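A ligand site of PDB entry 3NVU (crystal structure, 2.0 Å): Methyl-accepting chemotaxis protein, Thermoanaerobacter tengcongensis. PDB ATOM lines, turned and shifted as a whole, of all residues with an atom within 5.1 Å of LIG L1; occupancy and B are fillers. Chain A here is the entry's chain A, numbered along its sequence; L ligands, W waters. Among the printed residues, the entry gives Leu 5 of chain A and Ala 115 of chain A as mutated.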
ATOM      1  N   MET A   1      -7.796  -1.689  36.900  1.00  0.00           N
ATOM      2  CA  MET A   1      -7.949  -1.181  35.539  1.00  0.00           C
ATOM      3  C   MET A   1      -8.017  -2.319  34.527  1.00  0.00           C
ATOM      4  O   MET A   1      -7.179  -3.228  34.569  1.00  0.00           O
ATOM      5  CB  MET A   1      -6.800  -0.234  35.190  1.00  0.00           C
ATOM      6  CG  MET A   1      -6.972   0.471  33.837  1.00  0.00           C
ATOM      7  SD  MET A   1      -8.507   1.446  33.775  1.00  0.00           S
ATOM      8  CE  MET A   1      -8.048   2.822  34.847  1.00  0.00           C
ATOM      9  N   LYS A   2      -8.994  -2.271  33.635  1.00  0.00           N
ATOM     10  CA  LYS A   2      -9.134  -3.280  32.573  1.00  0.00           C
ATOM     11  C   LYS A   2      -7.853  -3.376  31.764  1.00  0.00           C
ATOM     12  O   LYS A   2      -7.192  -2.352  31.508  1.00  0.00           O
ATOM     13  CB  LYS A   2     -10.338  -2.978  31.664  1.00  0.00           C
ATOM     14  CG  LYS A   2     -10.702  -4.084  30.674  1.00  0.00           C
ATOM     15  CD  LYS A   2     -12.031  -3.819  29.941  1.00  0.00           C
ATOM     16  CE  LYS A   2     -12.403  -4.991  29.007  1.00  0.00           C
ATOM     17  NZ  LYS A   2     -13.589  -4.722  28.145  1.00  0.00           N
ATOM     18  N   THR A   4      -7.255  -3.713  28.711  1.00  0.00           N
ATOM     19  CA  THR A   4      -7.242  -2.990  27.458  1.00  0.00           C
ATOM     20  C   THR A   4      -6.379  -1.720  27.550  1.00  0.00           C
ATOM     21  O   THR A   4      -5.508  -1.475  26.724  1.00  0.00           O
ATOM     22  CB  THR A   4      -8.666  -2.613  27.002  1.00  0.00           C
ATOM     23  OG1 THR A   4      -9.466  -3.791  26.873  1.00  0.00           O
ATOM     24  CG2 THR A   4      -8.613  -1.882  25.663  1.00  0.00           C
ATOM     25  N   LEU A   5      -6.625  -0.900  28.570  1.00  0.00           N
ATOM     26  CA  LEU A   5      -5.848   0.320  28.728  1.00  0.00           C
ATOM     27  C   LEU A   5      -4.437   0.017  29.232  1.00  0.00           C
ATOM     28  O   LEU A   5      -3.458   0.638  28.803  1.00  0.00           O
ATOM     29  CB  LEU A   5      -6.555   1.291  29.669  1.00  0.00           C
ATOM     30  CG  LEU A   5      -5.935   2.685  29.820  1.00  0.00           C
ATOM     31  CD1 LEU A   5      -5.813   3.456  28.471  1.00  0.00           C
ATOM     32  CD2 LEU A   5      -6.749   3.500  30.835  1.00  0.00           C
ATOM     33  N   ILE A  75      -2.017   9.060  23.484  1.00  0.00           N
ATOM     34  CA  ILE A  75      -2.866   9.432  22.357  1.00  0.00           C
ATOM     35  C   ILE A  75      -2.298   8.879  21.046  1.00  0.00           C
ATOM     36  O   ILE A  75      -3.040   8.369  20.206  1.00  0.00           O
ATOM     37  CB  ILE A  75      -3.046  10.971  22.267  1.00  0.00           C
ATOM     38  CG1 ILE A  75      -3.869  11.490  23.468  1.00  0.00           C
ATOM     39  CG2 ILE A  75      -3.689  11.353  20.933  1.00  0.00           C
ATOM     40  CD1 ILE A  75      -5.301  10.972  23.490  1.00  0.00           C
ATOM     41  N   PHE A  78      -2.931   5.168  21.018  1.00  0.00           N
ATOM     42  CA  PHE A  78      -4.333   4.962  20.634  1.00  0.00           C
ATOM     43  C   PHE A  78      -4.508   5.092  19.123  1.00  0.00           C
ATOM     44  O   PHE A  78      -5.208   4.287  18.497  1.00  0.00           O
ATOM     45  CB  PHE A  78      -5.245   5.993  21.313  1.00  0.00           C
ATOM     46  CG  PHE A  78      -5.498   5.730  22.776  1.00  0.00           C
ATOM     47  CD1 PHE A  78      -5.780   6.800  23.636  1.00  0.00           C
ATOM     48  CD2 PHE A  78      -5.489   4.435  23.285  1.00  0.00           C
ATOM     49  CE1 PHE A  78      -6.036   6.575  24.992  1.00  0.00           C
ATOM     50  CE2 PHE A  78      -5.761   4.196  24.635  1.00  0.00           C
ATOM     51  CZ  PHE A  78      -6.031   5.271  25.497  1.00  0.00           C
ATOM     52  N   PHE A  82      -5.873   1.923  17.603  1.00  0.00           N
ATOM     53  CA  PHE A  82      -7.284   2.103  17.295  1.00  0.00           C
ATOM     54  C   PHE A  82      -7.503   3.341  16.451  1.00  0.00           C
ATOM     55  O   PHE A  82      -8.099   4.306  16.917  1.00  0.00           O
ATOM     56  CB  PHE A  82      -8.108   2.196  18.588  1.00  0.00           C
ATOM     57  CG  PHE A  82      -7.743   1.147  19.598  1.00  0.00           C
ATOM     58  CD1 PHE A  82      -7.130   1.494  20.798  1.00  0.00           C
ATOM     59  CD2 PHE A  82      -7.990  -0.201  19.343  1.00  0.00           C
ATOM     60  CE1 PHE A  82      -6.782   0.534  21.723  1.00  0.00           C
ATOM     61  CE2 PHE A  82      -7.645  -1.187  20.276  1.00  0.00           C
ATOM     62  CZ  PHE A  82      -7.041  -0.819  21.466  1.00  0.00           C
ATOM     63  N   TYR A  85     -10.886   5.603  15.882  1.00  0.00           N
ATOM     64  CA  TYR A  85     -11.376   6.704  16.702  1.00  0.00           C
ATOM     65  C   TYR A  85     -10.850   8.048  16.229  1.00  0.00           C
ATOM     66  O   TYR A  85     -11.320   9.086  16.672  1.00  0.00           O
ATOM     67  CB  TYR A  85     -10.973   6.514  18.161  1.00  0.00           C
ATOM     68  CG  TYR A  85     -11.682   5.370  18.837  1.00  0.00           C
ATOM     69  CD1 TYR A  85     -11.046   4.148  19.037  1.00  0.00           C
ATOM     70  CD2 TYR A  85     -12.994   5.506  19.272  1.00  0.00           C
ATOM     71  CE1 TYR A  85     -11.697   3.098  19.656  1.00  0.00           C
ATOM     72  CE2 TYR A  85     -13.653   4.472  19.889  1.00  0.00           C
ATOM     73  CZ  TYR A  85     -13.006   3.261  20.084  1.00  0.00           C
ATOM     74  OH  TYR A  85     -13.665   2.227  20.701  1.00  0.00           O
ATOM     75  N   PHE A  86      -9.870   8.026  15.325  1.00  0.00           N
ATOM     76  CA  PHE A  86      -9.218   9.275  14.914  1.00  0.00           C
ATOM     77  C   PHE A  86      -9.573   9.649  13.480  1.00  0.00           C
ATOM     78  O   PHE A  86      -9.630  10.834  13.136  1.00  0.00           O
ATOM     79  CB  PHE A  86      -7.694   9.153  15.061  1.00  0.00           C
ATOM     80  CG  PHE A  86      -7.238   9.013  16.482  1.00  0.00           C
ATOM     81  CD1 PHE A  86      -6.793  10.130  17.203  1.00  0.00           C
ATOM     82  CD2 PHE A  86      -7.271   7.782  17.122  1.00  0.00           C
ATOM     83  CE1 PHE A  86      -6.369  10.006  18.509  1.00  0.00           C
ATOM     84  CE2 PHE A  86      -6.843   7.661  18.441  1.00  0.00           C
ATOM     85  CZ  PHE A  86      -6.401   8.762  19.129  1.00  0.00           C
ATOM     86  N   PHE A  94     -13.482  15.359  18.401  1.00  0.00           N
ATOM     87  CA  PHE A  94     -12.830  14.256  19.091  1.00  0.00           C
ATOM     88  C   PHE A  94     -13.033  14.394  20.606  1.00  0.00           C
ATOM     89  O   PHE A  94     -13.524  13.470  21.277  1.00  0.00           O
ATOM     90  CB  PHE A  94     -11.343  14.223  18.739  1.00  0.00           C
ATOM     91  CG  PHE A  94     -10.571  13.142  19.458  1.00  0.00           C
ATOM     92  CD1 PHE A  94     -10.510  11.857  18.941  1.00  0.00           C
ATOM     93  CD2 PHE A  94      -9.875  13.424  20.628  1.00  0.00           C
ATOM     94  CE1 PHE A  94      -9.784  10.858  19.589  1.00  0.00           C
ATOM     95  CE2 PHE A  94      -9.145  12.428  21.289  1.00  0.00           C
ATOM     96  CZ  PHE A  94      -9.094  11.151  20.766  1.00  0.00           C
ATOM     97  N   LEU A  95     -12.686  15.550  21.154  1.00  0.00           N
ATOM     98  CA  LEU A  95     -12.868  15.769  22.573  1.00  0.00           C
ATOM     99  C   LEU A  95     -14.350  15.626  22.933  1.00  0.00           C
ATOM    100  O   LEU A  95     -14.709  15.017  23.946  1.00  0.00           O
ATOM    101  CB  LEU A  95     -12.355  17.146  22.981  1.00  0.00           C
ATOM    102  CG  LEU A  95     -10.831  17.273  22.878  1.00  0.00           C
ATOM    103  CD1 LEU A  95     -10.396  18.684  23.213  1.00  0.00           C
ATOM    104  CD2 LEU A  95     -10.141  16.267  23.801  1.00  0.00           C
ATOM    105  N   MET A  98     -15.542  12.058  23.493  1.00  0.00           N
ATOM    106  CA  MET A  98     -14.818  11.190  24.426  1.00  0.00           C
ATOM    107  C   MET A  98     -15.704  10.508  25.481  1.00  0.00           C
ATOM    108  O   MET A  98     -15.542   9.314  25.790  1.00  0.00           O
ATOM    109  CB  MET A  98     -13.636  11.928  25.073  1.00  0.00           C
ATOM    110  CG  MET A  98     -12.425  12.055  24.152  1.00  0.00           C
ATOM    111  SD  MET A  98     -11.888  10.414  23.594  1.00  0.00           S
ATOM    112  CE  MET A  98     -12.477  10.371  21.901  1.00  0.00           C
ATOM    113  N   VAL A 101     -17.525   7.644  23.822  1.00  0.00           N
ATOM    114  CA  VAL A 101     -16.578   6.573  23.494  1.00  0.00           C
ATOM    115  C   VAL A 101     -16.235   5.745  24.730  1.00  0.00           C
ATOM    116  O   VAL A 101     -16.183   4.509  24.673  1.00  0.00           O
ATOM    117  CB  VAL A 101     -15.313   7.141  22.853  1.00  0.00           C
ATOM    118  CG1 VAL A 101     -14.237   6.072  22.777  1.00  0.00           C
ATOM    119  CG2 VAL A 101     -15.648   7.689  21.464  1.00  0.00           C
ATOM    120  N   HIS A 102     -16.005   6.409  25.847  1.00  0.00           N
ATOM    121  CA  HIS A 102     -15.651   5.694  27.068  1.00  0.00           C
ATOM    122  C   HIS A 102     -16.830   4.920  27.649  1.00  0.00           C
ATOM    123  O   HIS A 102     -16.645   3.835  28.201  1.00  0.00           O
ATOM    124  CB  HIS A 102     -15.024   6.647  28.085  1.00  0.00           C
ATOM    125  CG  HIS A 102     -13.633   7.074  27.715  1.00  0.00           C
ATOM    126  ND1 HIS A 102     -13.378   7.939  26.665  1.00  0.00           N
ATOM    127  CD2 HIS A 102     -12.426   6.723  28.212  1.00  0.00           C
ATOM    128  CE1 HIS A 102     -12.077   8.119  26.561  1.00  0.00           C
ATOM    129  NE2 HIS A 102     -11.476   7.390  27.482  1.00  0.00           N
ATOM    130  N   LEU A 105     -16.935   1.677  25.967  1.00  0.00           N
ATOM    131  CA  LEU A 105     -15.869   0.807  26.449  1.00  0.00           C
ATOM    132  C   LEU A 105     -16.088   0.309  27.877  1.00  0.00           C
ATOM    133  O   LEU A 105     -15.486  -0.679  28.290  1.00  0.00           O
ATOM    134  CB  LEU A 105     -14.509   1.524  26.361  1.00  0.00           C
ATOM    135  CG  LEU A 105     -14.026   1.882  24.955  1.00  0.00           C
ATOM    136  CD1 LEU A 105     -12.740   2.693  25.011  1.00  0.00           C
ATOM    137  CD2 LEU A 105     -13.850   0.634  24.120  1.00  0.00           C
ATOM    138  N   THR A 106     -16.933   0.999  28.641  1.00  0.00           N
ATOM    139  CA  THR A 106     -17.174   0.635  30.039  1.00  0.00           C
ATOM    140  C   THR A 106     -18.590   0.087  30.276  1.00  0.00           C
ATOM    141  O   THR A 106     -18.952  -0.215  31.411  1.00  0.00           O
ATOM    142  CB  THR A 106     -16.880   1.823  31.020  1.00  0.00           C
ATOM    143  OG1 THR A 106     -17.848   2.873  30.838  1.00  0.00           O
ATOM    144  CG2 THR A 106     -15.457   2.364  30.812  1.00  0.00           C
ATOM    145  N   ILE A 109     -18.592  -3.375  32.493  1.00  0.00           N
ATOM    146  CA  ILE A 109     -17.725  -3.518  33.653  1.00  0.00           C
ATOM    147  C   ILE A 109     -18.542  -3.834  34.915  1.00  0.00           C
ATOM    148  O   ILE A 109     -19.732  -3.519  34.989  1.00  0.00           O
ATOM    149  CB  ILE A 109     -16.862  -2.253  33.886  1.00  0.00           C
ATOM    150  CG1 ILE A 109     -16.091  -1.889  32.614  1.00  0.00           C
ATOM    151  CG2 ILE A 109     -15.881  -2.477  35.024  1.00  0.00           C
ATOM    152  CD1 ILE A 109     -14.905  -2.797  32.324  1.00  0.00           C
ATOM    153  N   ALA A 115     -16.649   6.282  35.111  1.00  0.00           N
ATOM    154  CA  ALA A 115     -15.892   7.527  34.979  1.00  0.00           C
ATOM    155  C   ALA A 115     -16.534   8.346  33.859  1.00  0.00           C
ATOM    156  O   ALA A 115     -17.013   7.781  32.869  1.00  0.00           O
ATOM    157  CB  ALA A 115     -14.434   7.224  34.653  1.00  0.00           C
ATOM    158  N   LEU A 117     -16.430  11.895  31.179  1.00  0.00           N
ATOM    159  CA  LEU A 117     -15.599  12.908  30.543  1.00  0.00           C
ATOM    160  C   LEU A 117     -16.474  13.967  29.851  1.00  0.00           C
ATOM    161  O   LEU A 117     -16.222  14.363  28.710  1.00  0.00           O
ATOM    162  CB  LEU A 117     -14.605  12.285  29.558  1.00  0.00           C
ATOM    163  CG  LEU A 117     -13.597  11.291  30.150  1.00  0.00           C
ATOM    164  CD1 LEU A 117     -12.846  10.593  29.015  1.00  0.00           C
ATOM    165  CD2 LEU A 117     -12.596  11.966  31.121  1.00  0.00           C
ATOM    166  N   MET A 129     -14.435  20.736  30.143  1.00  0.00           N
ATOM    167  CA  MET A 129     -14.415  19.283  30.170  1.00  0.00           C
ATOM    168  C   MET A 129     -14.190  18.846  31.611  1.00  0.00           C
ATOM    169  O   MET A 129     -13.233  19.301  32.249  1.00  0.00           O
ATOM    170  CB  MET A 129     -13.315  18.742  29.266  1.00  0.00           C
ATOM    171  CG  MET A 129     -13.510  17.301  28.860  1.00  0.00           C
ATOM    172  SD  MET A 129     -12.377  16.866  27.529  1.00  0.00           S
ATOM    173  CE  MET A 129     -12.890  15.190  27.160  1.00  0.00           C
ATOM    174  N   TYR A 131     -13.537  15.781  34.218  1.00  0.00           N
ATOM    175  CA  TYR A 131     -13.165  14.419  34.529  1.00  0.00           C
ATOM    176  C   TYR A 131     -13.733  14.037  35.886  1.00  0.00           C
ATOM    177  O   TYR A 131     -13.370  14.624  36.897  1.00  0.00           O
ATOM    178  CB  TYR A 131     -11.650  14.345  34.576  1.00  0.00           C
ATOM    179  CG  TYR A 131     -11.112  13.058  35.134  1.00  0.00           C
ATOM    180  CD1 TYR A 131     -11.704  11.842  34.840  1.00  0.00           C
ATOM    181  CD2 TYR A 131      -9.974  13.050  35.929  1.00  0.00           C
ATOM    182  CE1 TYR A 131     -11.193  10.661  35.337  1.00  0.00           C
ATOM    183  CE2 TYR A 131      -9.458  11.890  36.427  1.00  0.00           C
ATOM    184  CZ  TYR A 131     -10.059  10.696  36.124  1.00  0.00           C
ATOM    185  OH  TYR A 131      -9.521   9.548  36.650  1.00  0.00           O
ATOM    186  N   SER A 133     -14.371  10.712  38.474  1.00  0.00           N
ATOM    187  CA  SER A 133     -14.014   9.314  38.730  1.00  0.00           C
ATOM    188  C   SER A 133     -13.718   9.067  40.194  1.00  0.00           C
ATOM    189  O   SER A 133     -13.798   9.975  41.027  1.00  0.00           O
ATOM    190  CB  SER A 133     -12.789   8.907  37.889  1.00  0.00           C
ATOM    191  OG  SER A 133     -12.331   7.609  38.263  1.00  0.00           O
ATOM    192  N   ARG A 135     -10.772   7.349  40.725  1.00  0.00           N
ATOM    193  CA  ARG A 135      -9.338   7.061  40.627  1.00  0.00           C
ATOM    194  C   ARG A 135      -8.376   8.263  40.707  1.00  0.00           C
ATOM    195  O   ARG A 135      -7.179   8.091  40.936  1.00  0.00           O
ATOM    196  CB  ARG A 135      -9.053   6.302  39.341  1.00  0.00           C
ATOM    197  CG  ARG A 135      -9.350   4.820  39.403  1.00  0.00           C
ATOM    198  CD  ARG A 135      -8.761   4.116  38.196  1.00  0.00           C
ATOM    199  NE  ARG A 135      -9.003   2.681  38.266  1.00  0.00           N
ATOM    200  CZ  ARG A 135      -9.986   2.053  37.632  1.00  0.00           C
ATOM    201  NH1 ARG A 135     -10.824   2.747  36.871  1.00  0.00           N
ATOM    202  NH2 ARG A 135     -10.129   0.739  37.762  1.00  0.00           N
ATOM    203  N   LYS A 136      -8.881   9.464  40.495  1.00  0.00           N
ATOM    204  CA  LYS A 136      -8.025  10.651  40.656  1.00  0.00           C
ATOM    205  C   LYS A 136      -6.798  10.708  39.700  1.00  0.00           C
ATOM    206  O   LYS A 136      -5.704  11.118  40.085  1.00  0.00           O
ATOM    207  CB  LYS A 136      -7.558  10.750  42.118  1.00  0.00           C
ATOM    208  CG  LYS A 136      -6.921  12.081  42.476  1.00  0.00           C
ATOM    209  CD  LYS A 136      -6.072  12.020  43.763  1.00  0.00           C
ATOM    210  CE  LYS A 136      -6.892  12.344  45.009  1.00  0.00           C
ATOM    211  NZ  LYS A 136      -7.823  11.252  45.337  1.00  0.00           N
ATOM    212  N   MET A 137      -6.971  10.307  38.441  1.00  0.00           N
ATOM    213  CA  MET A 137      -5.857  10.367  37.494  1.00  0.00           C
ATOM    214  C   MET A 137      -5.674  11.747  36.851  1.00  0.00           C
ATOM    215  O   MET A 137      -5.730  11.892  35.616  1.00  0.00           O
ATOM    216  CB  MET A 137      -6.024   9.281  36.436  1.00  0.00           C
ATOM    217  CG  MET A 137      -6.180   7.900  37.062  1.00  0.00           C
ATOM    218  SD  MET A 137      -6.258   6.589  35.825  1.00  0.00           S
ATOM    219  CE  MET A 137      -4.510   6.396  35.424  1.00  0.00           C
ATOM    220  N   TYR A 140      -2.747  12.300  34.278  1.00  0.00           N
ATOM    221  CA  TYR A 140      -3.018  11.497  33.092  1.00  0.00           C
ATOM    222  C   TYR A 140      -4.035  12.211  32.184  1.00  0.00           C
ATOM    223  O   TYR A 140      -3.836  12.365  30.972  1.00  0.00           O
ATOM    224  CB  TYR A 140      -3.532  10.105  33.534  1.00  0.00           C
ATOM    225  CG  TYR A 140      -3.814   9.132  32.399  1.00  0.00           C
ATOM    226  CD1 TYR A 140      -2.809   8.783  31.500  1.00  0.00           C
ATOM    227  CD2 TYR A 140      -5.078   8.545  32.253  1.00  0.00           C
ATOM    228  CE1 TYR A 140      -3.043   7.896  30.458  1.00  0.00           C
ATOM    229  CE2 TYR A 140      -5.332   7.636  31.201  1.00  0.00           C
ATOM    230  CZ  TYR A 140      -4.305   7.322  30.309  1.00  0.00           C
ATOM    231  OH  TYR A 140      -4.518   6.440  29.267  1.00  0.00           O
ATOM    232  N   PHE A 141      -5.138  12.637  32.778  1.00  0.00           N
ATOM    233  CA  PHE A 141      -6.188  13.386  32.088  1.00  0.00           C
ATOM    234  C   PHE A 141      -5.645  14.622  31.365  1.00  0.00           C
ATOM    235  O   PHE A 141      -5.916  14.839  30.176  1.00  0.00           O
ATOM    236  CB  PHE A 141      -7.256  13.783  33.098  1.00  0.00           C
ATOM    237  CG  PHE A 141      -8.323  14.705  32.543  1.00  0.00           C
ATOM    238  CD1 PHE A 141      -9.161  14.298  31.522  1.00  0.00           C
ATOM    239  CD2 PHE A 141      -8.510  15.963  33.088  1.00  0.00           C
ATOM    240  CE1 PHE A 141     -10.156  15.124  31.025  1.00  0.00           C
ATOM    241  CE2 PHE A 141      -9.518  16.815  32.599  1.00  0.00           C
ATOM    242  CZ  PHE A 141     -10.332  16.393  31.564  1.00  0.00           C
ATOM    243  N   LEU A 144      -3.488  13.528  28.401  1.00  0.00           N
ATOM    244  CA  LEU A 144      -4.290  13.112  27.261  1.00  0.00           C
ATOM    245  C   LEU A 144      -4.841  14.315  26.474  1.00  0.00           C
ATOM    246  O   LEU A 144      -4.898  14.300  25.246  1.00  0.00           O
ATOM    247  CB  LEU A 144      -5.454  12.202  27.707  1.00  0.00           C
ATOM    248  CG  LEU A 144      -5.087  10.826  28.261  1.00  0.00           C
ATOM    249  CD1 LEU A 144      -6.227  10.296  29.180  1.00  0.00           C
ATOM    250  CD2 LEU A 144      -4.780   9.849  27.133  1.00  0.00           C
ATOM    251  N   ILE A 145      -5.247  15.374  27.181  1.00  0.00           N
ATOM    252  CA  ILE A 145      -5.720  16.569  26.483  1.00  0.00           C
ATOM    253  C   ILE A 145      -4.589  17.189  25.647  1.00  0.00           C
ATOM    254  O   ILE A 145      -4.775  17.487  24.470  1.00  0.00           O
ATOM    255  CB  ILE A 145      -6.309  17.599  27.454  1.00  0.00           C
ATOM    256  CG1 ILE A 145      -7.586  17.044  28.081  1.00  0.00           C
ATOM    257  CG2 ILE A 145      -6.626  18.925  26.717  1.00  0.00           C
ATOM    258  CD1 ILE A 145      -8.012  17.791  29.336  1.00  0.00           C
ATOM    259  N   SER A 148      -3.823  15.106  22.652  1.00  0.00           N
ATOM    260  CA  SER A 148      -4.849  15.257  21.630  1.00  0.00           C
ATOM    261  C   SER A 148      -4.550  16.468  20.754  1.00  0.00           C
ATOM    262  O   SER A 148      -4.545  16.360  19.518  1.00  0.00           O
ATOM    263  CB  SER A 148      -6.229  15.399  22.295  1.00  0.00           C
ATOM    264  OG  SER A 148      -6.584  14.195  22.982  1.00  0.00           O
HETATM  265  C1  LIG L   1      -9.814   5.376  30.710  1.00  0.00           C
HETATM  266  C2  LIG L   1      -9.644   4.355  25.978  1.00  0.00           C
HETATM  267  C3  LIG L   1      -8.943   9.000  24.815  1.00  0.00           C
HETATM  268  C4  LIG L   1      -9.432  10.093  29.467  1.00  0.00           C
HETATM  269  C5  LIG L   1      -9.849   4.673  29.525  1.00  0.00           C
HETATM  270  C6  LIG L   1     -10.080   3.268  29.362  1.00  0.00           C
HETATM  271  C7  LIG L   1     -10.040   2.980  28.055  1.00  0.00           C
HETATM  272  C8  LIG L   1      -9.773   4.211  27.339  1.00  0.00           C
HETATM  273  C9  LIG L   1     -10.233   1.574  27.456  1.00  0.00           C
HETATM  274  C10 LIG L   1     -10.349   2.220  30.466  1.00  0.00           C
HETATM  275  C11 LIG L   1     -11.707   2.505  31.098  1.00  0.00           C
HETATM  276  C12 LIG L   1     -11.995   1.442  32.113  1.00  0.00           C
HETATM  277  O1  LIG L   1     -12.185   1.792  33.305  1.00  0.00           O
HETATM  278  O2  LIG L   1     -12.022   0.251  31.728  1.00  0.00           O
HETATM  279  C13 LIG L   1      -9.455   5.516  25.268  1.00  0.00           C
HETATM  280  C14 LIG L   1      -9.368   5.596  23.813  1.00  0.00           C
HETATM  281  C15 LIG L   1      -9.169   6.881  23.501  1.00  0.00           C
HETATM  282  C16 LIG L   1      -9.149   7.649  24.730  1.00  0.00           C
HETATM  283  C17 LIG L   1      -9.467   4.375  22.862  1.00  0.00           C
HETATM  284  C18 LIG L   1      -9.002   7.542  22.100  1.00  0.00           C
HETATM  285  C19 LIG L   1      -9.229   6.878  20.958  1.00  0.00           C
HETATM  286  C20 LIG L   1      -9.043   9.712  25.969  1.00  0.00           C
HETATM  287  C21 LIG L   1      -9.011  11.147  26.089  1.00  0.00           C
HETATM  288  C22 LIG L   1      -9.156  11.454  27.390  1.00  0.00           C
HETATM  289  C23 LIG L   1      -9.284  10.214  28.112  1.00  0.00           C
HETATM  290  C24 LIG L   1      -8.841  12.111  24.901  1.00  0.00           C
HETATM  291  C25 LIG L   1      -9.198  12.847  28.068  1.00  0.00           C
HETATM  292  C26 LIG L   1      -9.182  13.983  27.371  1.00  0.00           C
HETATM  293  C27 LIG L   1      -9.435   8.947  30.216  1.00  0.00           C
HETATM  294  C28 LIG L   1      -9.187   8.918  31.646  1.00  0.00           C
HETATM  295  C29 LIG L   1      -9.274   7.448  32.038  1.00  0.00           C
HETATM  296  C30 LIG L   1      -9.601   6.737  30.813  1.00  0.00           C
HETATM  297  C31 LIG L   1      -8.869  10.108  32.565  1.00  0.00           C
HETATM  298  C32 LIG L   1      -9.141   6.868  33.453  1.00  0.00           C
HETATM  299  C33 LIG L   1     -10.568   7.040  34.012  1.00  0.00           C
HETATM  300  C34 LIG L   1     -10.742   6.378  35.355  1.00  0.00           C
HETATM  301  O3  LIG L   1     -10.381   6.979  36.386  1.00  0.00           O
HETATM  302  O4  LIG L   1     -11.277   5.237  35.408  1.00  0.00           O
HETATM  303  N1  LIG L   1      -9.673   5.225  28.268  1.00  0.00           N
HETATM  304  N2  LIG L   1      -9.317   6.782  25.788  1.00  0.00           N
HETATM  305  N3  LIG L   1      -9.220   9.160  27.226  1.00  0.00           N
HETATM  306  N4  LIG L   1      -9.677   7.647  29.763  1.00  0.00           N
HETATM  307 FE1  LIG L   1      -9.415   7.197  27.793  1.00  0.00          FE
HETATM  308  O1  LG2 L   2      -7.289   7.081  27.985  1.00  0.00           O
HETATM  309  O2  LG2 L   2      -7.174   6.162  29.023  1.00  0.00           O
HETATM  310  O   HOH W   1     -13.775   1.148  35.669  1.00  0.00           O
HETATM  311  O   HOH W   2     -12.115   5.151  38.152  1.00  0.00           O
HETATM  312  O   HOH W   3     -11.483  -0.654  34.325  1.00  0.00           O
HETATM  313  O   HOH W   4     -12.989   4.268  33.644  1.00  0.00           O
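FE1 of LIG L1 is bound by NE2 of His 102, at 2.1 Å.
O3 of LIG L1 lies within hydrogen-bond range of OH of Tyr 131, at 2.7 Å.
An oxygen (O3) of LIG L1 lies within hydrogen-bond range of the side-chain hydroxyl (OG) of Ser 133, at 2.8 Å.
The guanidinium group (NH1) of Arg 135 is in salt-bridge range of an oxygen (O4) of LIG L1 (2.9 Å).
OH of Tyr 140 is in hydrogen-bond range of O2 of LG2 L2 (2.7 Å).
FE1 of LIG L1 is bound by O1 of LG2 L2.
The backbone carbonyl oxygen (O) of Met 98 is in hydrogen-bond range of a ring nitrogen (ND1) of His 102 (2.7 Å).
The backbone carbonyl oxygen (O) of His 102 lies within hydrogen-bond range of the side-chain hydroxyl (OG1) of Thr 106.
The side-chain hydroxyl of Tyr 131 is in hydrogen-bond range of the backbone NH of Met 137.
The side-chain hydroxyl (OG) of Ser 133 is in hydrogen-bond range of the backbone NH (N) of Arg 135 (2.9 Å).
The backbone carbonyl oxygen (O) of Leu 144 lies within hydrogen-bond range of the side-chain hydroxyl (OG) of Ser 148, at 2.8 Å.
O1 of LIG L1 lies close to SD of Met 1, at 3.7 Å.
CB of Lys 2 touches O2 of LIG L1, 3.6 Å away.
CD2 of Leu 5 touches C5 of LIG L1, at 3.6 Å.
Ile 75 touches LIG L1.
Phe 78 touches LIG L1.
CB of Tyr 85 touches C19 of LIG L1, 3.3 Å away.
Phe 86 touches LIG L1 (CE2 to C19, 3.6 Å).
Phe 94 touches LIG L1.
Met 98 touches LIG L1.
Leu 105 touches LIG L1.
Thr 106 touches LIG L1.
CB of Ala 115 touches O4 of LIG L1 (3.8 Å).
Leu 117 touches LIG L1 (CD1 to C4, 3.5 Å).
Met 129 touches LIG L1 (CE to C26, 3.9 Å).
SD of Met 137 touches C32 of LIG L1, 3.7 Å away.
Phe 141 touches LIG L1.
Leu 144 touches LIG L1 (CD1 to C4, 3.2 Å).
Ile 145 touches LIG L1 (CG1 to C26, 3.5 Å).
OG of Ser 148 touches C24 of LIG L1, at 3.6 Å.
23 residues have an atom within 4 Å of LIG L1: Met 1, Lys 2, Leu 5, Ile 75, Phe 78, Tyr 85, Phe 86, Phe 94, Met 98, His 102, Leu 105, Thr 106, Ala 115, Leu 117, Met 129, Tyr 131, Ser 133, Arg 135, Met 137, Phe 141, Leu 144, Ile 145 and Ser 148.
Water W3 lies within hydrogen-bond range of O1 of LIG L1 (2.7 Å), N of Lys 2 (3.0 Å) and SD of Met 1 (3.7 Å).
Water W2 lies within hydrogen-bond range of OG of Ser 133 (2.5 Å), O4 of LIG L1 (2.9 Å) and NH1 of Arg 135 (3.0 Å).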
